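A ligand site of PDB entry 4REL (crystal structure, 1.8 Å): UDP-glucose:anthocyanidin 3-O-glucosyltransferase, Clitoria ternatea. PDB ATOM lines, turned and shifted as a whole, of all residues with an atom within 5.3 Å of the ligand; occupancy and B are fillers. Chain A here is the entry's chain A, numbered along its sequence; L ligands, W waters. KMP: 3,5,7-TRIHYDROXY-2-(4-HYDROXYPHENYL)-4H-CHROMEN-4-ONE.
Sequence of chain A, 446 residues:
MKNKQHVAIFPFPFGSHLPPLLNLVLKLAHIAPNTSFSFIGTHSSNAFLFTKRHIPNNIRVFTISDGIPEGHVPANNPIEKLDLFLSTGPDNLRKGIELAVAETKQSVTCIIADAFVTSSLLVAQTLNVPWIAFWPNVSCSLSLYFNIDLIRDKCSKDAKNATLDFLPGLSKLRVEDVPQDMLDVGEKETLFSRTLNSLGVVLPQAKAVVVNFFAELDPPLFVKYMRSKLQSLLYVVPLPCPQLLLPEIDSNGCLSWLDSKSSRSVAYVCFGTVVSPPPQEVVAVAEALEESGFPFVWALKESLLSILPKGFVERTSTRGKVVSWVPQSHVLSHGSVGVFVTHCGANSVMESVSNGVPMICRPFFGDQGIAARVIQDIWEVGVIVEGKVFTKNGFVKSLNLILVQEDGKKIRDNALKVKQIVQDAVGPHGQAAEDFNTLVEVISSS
The side-chain carboxylate (OD2) of Asp 367 sits at hydrogen-bond distance from the side-chain hydroxyl (OG) of Ser 141, at 3.3 Å.
Water W1 lies within hydrogen-bond range of OH of Tyr 145 (2.9 Å) and O29 of the ligand (2.9 Å).
Water W3 lies within hydrogen-bond range of N of Asp 181 (2.9 Å) and O29 of the ligand (3.1 Å).
Water W2 lies within hydrogen-bond range of the side-chain carboxylate of Asp 367 (2.9 Å) and an oxygen (O13) of the ligand (3.1 Å).
The side-chain carboxylate of Asp 367 lies within hydrogen-bond range of an oxygen (O30) of the ligand, 3.0 Å away.
An oxygen (O13) of the ligand is in hydrogen-bond range of the side-chain amide nitrogen (ND2) of Asn 137 (2.9 Å).
NE2 of His 17 lies within hydrogen-bond range of O27 of the ligand (2.5 Å).
OD2 of Asp 181 lies within hydrogen-bond range of O29 of the ligand (2.7 Å).
Pro 78 touches the ligand (O to C18, 3.9 Å).
Leu 82 touches the ligand.
Phe 116 touches the ligand.
OH of Tyr 145 touches C1 of the ligand (3.6 Å).
CB of Pro 179 touches O29 of the ligand, at 3.7 Å.
Phe 192 touches the ligand.
Leu 196 touches the ligand (CD2 to C6, 3.5 Å).
CE2 of Phe 365 touches C19 of the ligand (3.2 Å).
Gly 366 touches the ligand (CA to C6, 3.5 Å).
Along chain A the residues within 4 Å of the ligand span positions 17 to 367.
The nearest printed residue that does not touch the ligand is Phe 14 (4.002 Å).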
ATOM      1  N   PHE A  12      12.656  20.453  -4.547  1.00  0.00           N
ATOM      2  CA  PHE A  12      12.539  19.004  -4.645  1.00  0.00           C
ATOM      3  C   PHE A  12      13.998  18.551  -4.608  1.00  0.00           C
ATOM      4  O   PHE A  12      14.769  18.870  -5.518  1.00  0.00           O
ATOM      5  CB  PHE A  12      11.853  18.643  -5.961  1.00  0.00           C
ATOM      6  CG  PHE A  12      11.492  17.192  -6.104  1.00  0.00           C
ATOM      7  CD1 PHE A  12      10.688  16.537  -5.174  1.00  0.00           C
ATOM      8  CD2 PHE A  12      11.918  16.476  -7.215  1.00  0.00           C
ATOM      9  CE1 PHE A  12      10.345  15.188  -5.341  1.00  0.00           C
ATOM     10  CE2 PHE A  12      11.584  15.124  -7.382  1.00  0.00           C
ATOM     11  CZ  PHE A  12      10.797  14.494  -6.454  1.00  0.00           C
ATOM     12  N   PHE A  14      16.450  16.746  -5.300  1.00  0.00           N
ATOM     13  CA  PHE A  14      17.016  15.732  -6.190  1.00  0.00           C
ATOM     14  C   PHE A  14      17.598  16.341  -7.452  1.00  0.00           C
ATOM     15  O   PHE A  14      16.887  17.034  -8.185  1.00  0.00           O
ATOM     16  CB  PHE A  14      15.945  14.709  -6.538  1.00  0.00           C
ATOM     17  CG  PHE A  14      15.391  14.016  -5.339  1.00  0.00           C
ATOM     18  CD1 PHE A  14      16.092  12.961  -4.759  1.00  0.00           C
ATOM     19  CD2 PHE A  14      14.200  14.450  -4.764  1.00  0.00           C
ATOM     20  CE1 PHE A  14      15.592  12.335  -3.611  1.00  0.00           C
ATOM     21  CE2 PHE A  14      13.709  13.821  -3.615  1.00  0.00           C
ATOM     22  CZ  PHE A  14      14.413  12.772  -3.043  1.00  0.00           C
ATOM     23  N   SER A  16      18.382  17.320 -10.809  1.00  0.00           N
ATOM     24  CA  SER A  16      18.082  18.335 -11.815  1.00  0.00           C
ATOM     25  C   SER A  16      17.149  19.442 -11.326  1.00  0.00           C
ATOM     26  O   SER A  16      17.054  20.501 -11.944  1.00  0.00           O
ATOM     27  CB  SER A  16      17.470  17.680 -13.051  1.00  0.00           C
ATOM     28  OG  SER A  16      16.226  17.067 -12.727  1.00  0.00           O
ATOM     29  N   HIS A  17      16.468  19.206 -10.209  1.00  0.00           N
ATOM     30  CA  HIS A  17      15.602  20.239  -9.652  1.00  0.00           C
ATOM     31  C   HIS A  17      16.344  21.277  -8.826  1.00  0.00           C
ATOM     32  O   HIS A  17      15.788  22.324  -8.509  1.00  0.00           O
ATOM     33  CB  HIS A  17      14.495  19.621  -8.807  1.00  0.00           C
ATOM     34  CG  HIS A  17      13.495  18.848  -9.611  1.00  0.00           C
ATOM     35  ND1 HIS A  17      12.203  19.286  -9.785  1.00  0.00           N
ATOM     36  CD2 HIS A  17      13.613  17.701 -10.307  1.00  0.00           C
ATOM     37  CE1 HIS A  17      11.546  18.416 -10.534  1.00  0.00           C
ATOM     38  NE2 HIS A  17      12.386  17.460 -10.882  1.00  0.00           N
ATOM     39  N   PRO A  78      14.837   4.886  -9.555  1.00  0.00           N
ATOM     40  CA  PRO A  78      14.864   6.339  -9.392  1.00  0.00           C
ATOM     41  C   PRO A  78      13.683   6.907  -8.609  1.00  0.00           C
ATOM     42  O   PRO A  78      13.644   8.112  -8.400  1.00  0.00           O
ATOM     43  CB  PRO A  78      14.798   6.839 -10.837  1.00  0.00           C
ATOM     44  CG  PRO A  78      13.987   5.787 -11.543  1.00  0.00           C
ATOM     45  CD  PRO A  78      14.405   4.489 -10.911  1.00  0.00           C
ATOM     46  N   ILE A  79      12.746   6.076  -8.175  1.00  0.00           N
ATOM     47  CA  ILE A  79      11.559   6.602  -7.523  1.00  0.00           C
ATOM     48  C   ILE A  79      11.611   6.460  -5.997  1.00  0.00           C
ATOM     49  O   ILE A  79      11.013   7.264  -5.273  1.00  0.00           O
ATOM     50  CB  ILE A  79      10.272   5.960  -8.067  1.00  0.00           C
ATOM     51  CG1 ILE A  79      10.226   6.087  -9.590  1.00  0.00           C
ATOM     52  CG2 ILE A  79       9.036   6.636  -7.488  1.00  0.00           C
ATOM     53  CD1 ILE A  79      10.312   7.527 -10.068  1.00  0.00           C
ATOM     54  N   LEU A  82      12.607   9.426  -3.867  1.00  0.00           N
ATOM     55  CA  LEU A  82      11.583  10.464  -4.013  1.00  0.00           C
ATOM     56  C   LEU A  82      10.403  10.174  -3.086  1.00  0.00           C
ATOM     57  O   LEU A  82       9.939  11.060  -2.368  1.00  0.00           O
ATOM     58  CB  LEU A  82      11.068  10.571  -5.457  1.00  0.00           C
ATOM     59  CG  LEU A  82      12.017  10.553  -6.661  1.00  0.00           C
ATOM     60  CD1 LEU A  82      11.260  10.891  -7.939  1.00  0.00           C
ATOM     61  CD2 LEU A  82      13.186  11.472  -6.483  1.00  0.00           C
ATOM     62  N   PHE A 116       6.579  19.991  -6.967  1.00  0.00           N
ATOM     63  CA  PHE A 116       6.427  18.597  -6.538  1.00  0.00           C
ATOM     64  C   PHE A 116       6.348  18.467  -5.016  1.00  0.00           C
ATOM     65  O   PHE A 116       5.874  17.444  -4.509  1.00  0.00           O
ATOM     66  CB  PHE A 116       7.563  17.714  -7.052  1.00  0.00           C
ATOM     67  CG  PHE A 116       7.528  17.437  -8.538  1.00  0.00           C
ATOM     68  CD1 PHE A 116       6.458  17.870  -9.315  1.00  0.00           C
ATOM     69  CD2 PHE A 116       8.567  16.750  -9.144  1.00  0.00           C
ATOM     70  CE1 PHE A 116       6.428  17.623 -10.691  1.00  0.00           C
ATOM     71  CE2 PHE A 116       8.545  16.493 -10.525  1.00  0.00           C
ATOM     72  CZ  PHE A 116       7.476  16.934 -11.296  1.00  0.00           C
ATOM     73  N   TRP A 135       8.335  25.689 -11.332  1.00  0.00           N
ATOM     74  CA  TRP A 135       8.199  24.602 -12.309  1.00  0.00           C
ATOM     75  C   TRP A 135       9.424  24.500 -13.206  1.00  0.00           C
ATOM     76  O   TRP A 135       9.525  25.210 -14.210  1.00  0.00           O
ATOM     77  CB  TRP A 135       6.965  24.870 -13.183  1.00  0.00           C
ATOM     78  CG  TRP A 135       6.603  23.709 -14.062  1.00  0.00           C
ATOM     79  CD1 TRP A 135       6.881  23.561 -15.384  1.00  0.00           C
ATOM     80  CD2 TRP A 135       5.886  22.533 -13.667  1.00  0.00           C
ATOM     81  NE1 TRP A 135       6.379  22.363 -15.841  1.00  0.00           N
ATOM     82  CE2 TRP A 135       5.761  21.713 -14.805  1.00  0.00           C
ATOM     83  CE3 TRP A 135       5.331  22.094 -12.455  1.00  0.00           C
ATOM     84  CZ2 TRP A 135       5.104  20.485 -14.778  1.00  0.00           C
ATOM     85  CZ3 TRP A 135       4.685  20.871 -12.421  1.00  0.00           C
ATOM     86  CH2 TRP A 135       4.580  20.079 -13.584  1.00  0.00           C
ATOM     87  N   ASN A 137      10.314  21.849 -14.923  1.00  0.00           N
ATOM     88  CA  ASN A 137      10.137  20.741 -15.863  1.00  0.00           C
ATOM     89  C   ASN A 137       9.777  21.265 -17.225  1.00  0.00           C
ATOM     90  O   ASN A 137       9.874  22.472 -17.474  1.00  0.00           O
ATOM     91  CB  ASN A 137       9.069  19.808 -15.312  1.00  0.00           C
ATOM     92  CG  ASN A 137       9.164  19.702 -13.811  1.00  0.00           C
ATOM     93  OD1 ASN A 137       8.265  20.138 -13.065  1.00  0.00           O
ATOM     94  ND2 ASN A 137      10.301  19.187 -13.347  1.00  0.00           N
ATOM     95  N   SER A 141       4.129  20.464 -20.045  1.00  0.00           N
ATOM     96  CA  SER A 141       3.544  19.352 -19.307  1.00  0.00           C
ATOM     97  C   SER A 141       2.588  19.834 -18.220  1.00  0.00           C
ATOM     98  O   SER A 141       1.800  19.058 -17.706  1.00  0.00           O
ATOM     99  CB  SER A 141       4.620  18.417 -18.751  1.00  0.00           C
ATOM    100  OG  SER A 141       5.303  19.034 -17.682  1.00  0.00           O
ATOM    101  N   TYR A 145      -1.788  17.940 -16.060  1.00  0.00           N
ATOM    102  CA  TYR A 145      -2.293  17.725 -14.704  1.00  0.00           C
ATOM    103  C   TYR A 145      -3.687  18.277 -14.466  1.00  0.00           C
ATOM    104  O   TYR A 145      -4.331  17.969 -13.463  1.00  0.00           O
ATOM    105  CB  TYR A 145      -1.249  18.224 -13.690  1.00  0.00           C
ATOM    106  CG  TYR A 145       0.033  17.448 -13.889  1.00  0.00           C
ATOM    107  CD1 TYR A 145       0.120  16.137 -13.472  1.00  0.00           C
ATOM    108  CD2 TYR A 145       1.106  18.004 -14.575  1.00  0.00           C
ATOM    109  CE1 TYR A 145       1.266  15.387 -13.692  1.00  0.00           C
ATOM    110  CE2 TYR A 145       2.265  17.265 -14.796  1.00  0.00           C
ATOM    111  CZ  TYR A 145       2.329  15.958 -14.345  1.00  0.00           C
ATOM    112  OH  TYR A 145       3.463  15.204 -14.559  1.00  0.00           O
ATOM    113  N   PRO A 179       3.375  10.890 -19.871  1.00  0.00           N
ATOM    114  CA  PRO A 179       4.162  10.235 -18.816  1.00  0.00           C
ATOM    115  C   PRO A 179       3.435   8.995 -18.281  1.00  0.00           C
ATOM    116  O   PRO A 179       2.257   9.087 -17.926  1.00  0.00           O
ATOM    117  CB  PRO A 179       4.239  11.305 -17.718  1.00  0.00           C
ATOM    118  CG  PRO A 179       4.186  12.598 -18.475  1.00  0.00           C
ATOM    119  CD  PRO A 179       3.201  12.332 -19.598  1.00  0.00           C
ATOM    120  N   ASP A 181       3.729   7.578 -15.521  1.00  0.00           N
ATOM    121  CA  ASP A 181       3.368   7.806 -14.118  1.00  0.00           C
ATOM    122  C   ASP A 181       1.913   8.247 -13.937  1.00  0.00           C
ATOM    123  O   ASP A 181       1.264   7.870 -12.958  1.00  0.00           O
ATOM    124  CB  ASP A 181       4.284   8.846 -13.453  1.00  0.00           C
ATOM    125  CG  ASP A 181       5.691   8.324 -13.192  1.00  0.00           C
ATOM    126  OD1 ASP A 181       5.863   7.123 -12.925  1.00  0.00           O
ATOM    127  OD2 ASP A 181       6.633   9.140 -13.249  1.00  0.00           O
ATOM    128  N   MET A 182       1.395   9.043 -14.869  1.00  0.00           N
ATOM    129  CA  MET A 182       0.074   9.622 -14.666  1.00  0.00           C
ATOM    130  C   MET A 182      -1.035   8.673 -15.073  1.00  0.00           C
ATOM    131  O   MET A 182      -2.204   8.903 -14.770  1.00  0.00           O
ATOM    132  CB  MET A 182      -0.072  11.009 -15.310  1.00  0.00           C
ATOM    133  CG  MET A 182      -0.239  11.029 -16.815  1.00  0.00           C
ATOM    134  SD  MET A 182      -0.586  12.732 -17.383  1.00  0.00           S
ATOM    135  CE  MET A 182      -2.134  13.046 -16.567  1.00  0.00           C
ATOM    136  N   PHE A 192       5.013   9.223  -5.214  1.00  0.00           N
ATOM    137  CA  PHE A 192       5.462  10.233  -6.174  1.00  0.00           C
ATOM    138  C   PHE A 192       4.415  10.446  -7.271  1.00  0.00           C
ATOM    139  O   PHE A 192       4.079  11.586  -7.588  1.00  0.00           O
ATOM    140  CB  PHE A 192       6.809   9.836  -6.767  1.00  0.00           C
ATOM    141  CG  PHE A 192       7.313  10.772  -7.825  1.00  0.00           C
ATOM    142  CD1 PHE A 192       7.663  12.081  -7.521  1.00  0.00           C
ATOM    143  CD2 PHE A 192       7.457  10.335  -9.134  1.00  0.00           C
ATOM    144  CE1 PHE A 192       8.137  12.934  -8.494  1.00  0.00           C
ATOM    145  CE2 PHE A 192       7.923  11.188 -10.123  1.00  0.00           C
ATOM    146  CZ  PHE A 192       8.269  12.494  -9.797  1.00  0.00           C
ATOM    147  N   LEU A 196       2.245  13.939  -8.065  1.00  0.00           N
ATOM    148  CA  LEU A 196       2.149  14.604  -9.355  1.00  0.00           C
ATOM    149  C   LEU A 196       0.691  14.701  -9.812  1.00  0.00           C
ATOM    150  O   LEU A 196       0.246  15.749 -10.286  1.00  0.00           O
ATOM    151  CB  LEU A 196       3.022  13.918 -10.419  1.00  0.00           C
ATOM    152  CG  LEU A 196       4.424  14.538 -10.567  1.00  0.00           C
ATOM    153  CD1 LEU A 196       5.163  14.614  -9.234  1.00  0.00           C
ATOM    154  CD2 LEU A 196       5.250  13.770 -11.577  1.00  0.00           C
ATOM    155  N   VAL A 274      19.773   9.695 -14.759  1.00  0.00           N
ATOM    156  CA  VAL A 274      18.685   9.358 -13.840  1.00  0.00           C
ATOM    157  C   VAL A 274      18.111   7.962 -14.080  1.00  0.00           C
ATOM    158  O   VAL A 274      17.861   7.208 -13.137  1.00  0.00           O
ATOM    159  CB  VAL A 274      17.570  10.428 -13.839  1.00  0.00           C
ATOM    160  CG1 VAL A 274      16.270   9.871 -13.256  1.00  0.00           C
ATOM    161  CG2 VAL A 274      18.025  11.668 -13.055  1.00  0.00           C
ATOM    162  N   PHE A 365      11.945   8.830 -19.799  1.00  0.00           N
ATOM    163  CA  PHE A 365      11.376   8.894 -18.468  1.00  0.00           C
ATOM    164  C   PHE A 365      10.582  10.186 -18.261  1.00  0.00           C
ATOM    165  O   PHE A 365      10.900  11.205 -18.865  1.00  0.00           O
ATOM    166  CB  PHE A 365      12.550   8.815 -17.480  1.00  0.00           C
ATOM    167  CG  PHE A 365      12.168   8.972 -16.045  1.00  0.00           C
ATOM    168  CD1 PHE A 365      11.803   7.869 -15.300  1.00  0.00           C
ATOM    169  CD2 PHE A 365      12.208  10.211 -15.440  1.00  0.00           C
ATOM    170  CE1 PHE A 365      11.456   7.994 -13.964  1.00  0.00           C
ATOM    171  CE2 PHE A 365      11.856  10.357 -14.115  1.00  0.00           C
ATOM    172  CZ  PHE A 365      11.478   9.243 -13.370  1.00  0.00           C
ATOM    173  N   GLY A 366       9.566  10.151 -17.412  1.00  0.00           N
ATOM    174  CA  GLY A 366       8.878  11.374 -16.998  1.00  0.00           C
ATOM    175  C   GLY A 366       8.244  12.153 -18.137  1.00  0.00           C
ATOM    176  O   GLY A 366       7.523  11.584 -18.957  1.00  0.00           O
ATOM    177  N   ASP A 367       8.497  13.464 -18.170  1.00  0.00           N
ATOM    178  CA  ASP A 367       7.943  14.308 -19.228  1.00  0.00           C
ATOM    179  C   ASP A 367       8.894  14.514 -20.415  1.00  0.00           C
ATOM    180  O   ASP A 367       8.698  15.415 -21.220  1.00  0.00           O
ATOM    181  CB  ASP A 367       7.450  15.669 -18.689  1.00  0.00           C
ATOM    182  CG  ASP A 367       8.570  16.530 -18.115  1.00  0.00           C
ATOM    183  OD1 ASP A 367       9.748  16.128 -18.136  1.00  0.00           O
ATOM    184  OD2 ASP A 367       8.267  17.659 -17.659  1.00  0.00           O
HETATM  185  C1  KMP L   1       6.721  13.622 -14.932  1.00  0.00           C
HETATM  186  C2  KMP L   1       7.666  14.622 -14.798  1.00  0.00           C
HETATM  187  C3  KMP L   1       8.888  14.352 -14.003  1.00  0.00           C
HETATM  188  C4  KMP L   1       9.072  13.026 -13.382  1.00  0.00           C
HETATM  189  C5  KMP L   1       8.064  12.078 -13.573  1.00  0.00           C
HETATM  190  C6  KMP L   1       6.917  12.379 -14.325  1.00  0.00           C
HETATM  191  C9  KMP L   1       9.930  15.384 -13.832  1.00  0.00           C
HETATM  192  C10 KMP L   1      11.119  15.030 -13.018  1.00  0.00           C
HETATM  193  C11 KMP L   1      11.203  13.658 -12.432  1.00  0.00           C
HETATM  194  C14 KMP L   1      12.366  13.209 -11.603  1.00  0.00           C
HETATM  195  C15 KMP L   1      13.307  14.105 -11.105  1.00  0.00           C
HETATM  196  C16 KMP L   1      14.374  13.656 -10.341  1.00  0.00           C
HETATM  197  C17 KMP L   1      14.519  12.299 -10.077  1.00  0.00           C
HETATM  198  C18 KMP L   1      13.578  11.403 -10.574  1.00  0.00           C
HETATM  199  C19 KMP L   1      12.510  11.854 -11.325  1.00  0.00           C
HETATM  200  O12 KMP L   1      10.192  12.737 -12.642  1.00  0.00           O
HETATM  201  O13 KMP L   1       9.801  16.519 -14.358  1.00  0.00           O
HETATM  202  O24 KMP L   1      15.572  11.866  -9.330  1.00  0.00           O
HETATM  203  O27 KMP L   1      12.099  15.972 -12.864  1.00  0.00           O
HETATM  204  O29 KMP L   1       5.962  11.416 -14.473  1.00  0.00           O
HETATM  205  O30 KMP L   1       7.492  15.841 -15.377  1.00  0.00           O
HETATM  206  O   HOH W   1       3.177  12.336 -14.411  1.00  0.00           O
HETATM  207  O   HOH W   2      11.446  17.941 -16.567  1.00  0.00           O
HETATM  208  O   HOH W   3       6.273   8.847 -16.122  1.00  0.00           O
HETATM  209  O   HOH W   4      18.033  12.961  -9.302  1.00  0.00           O
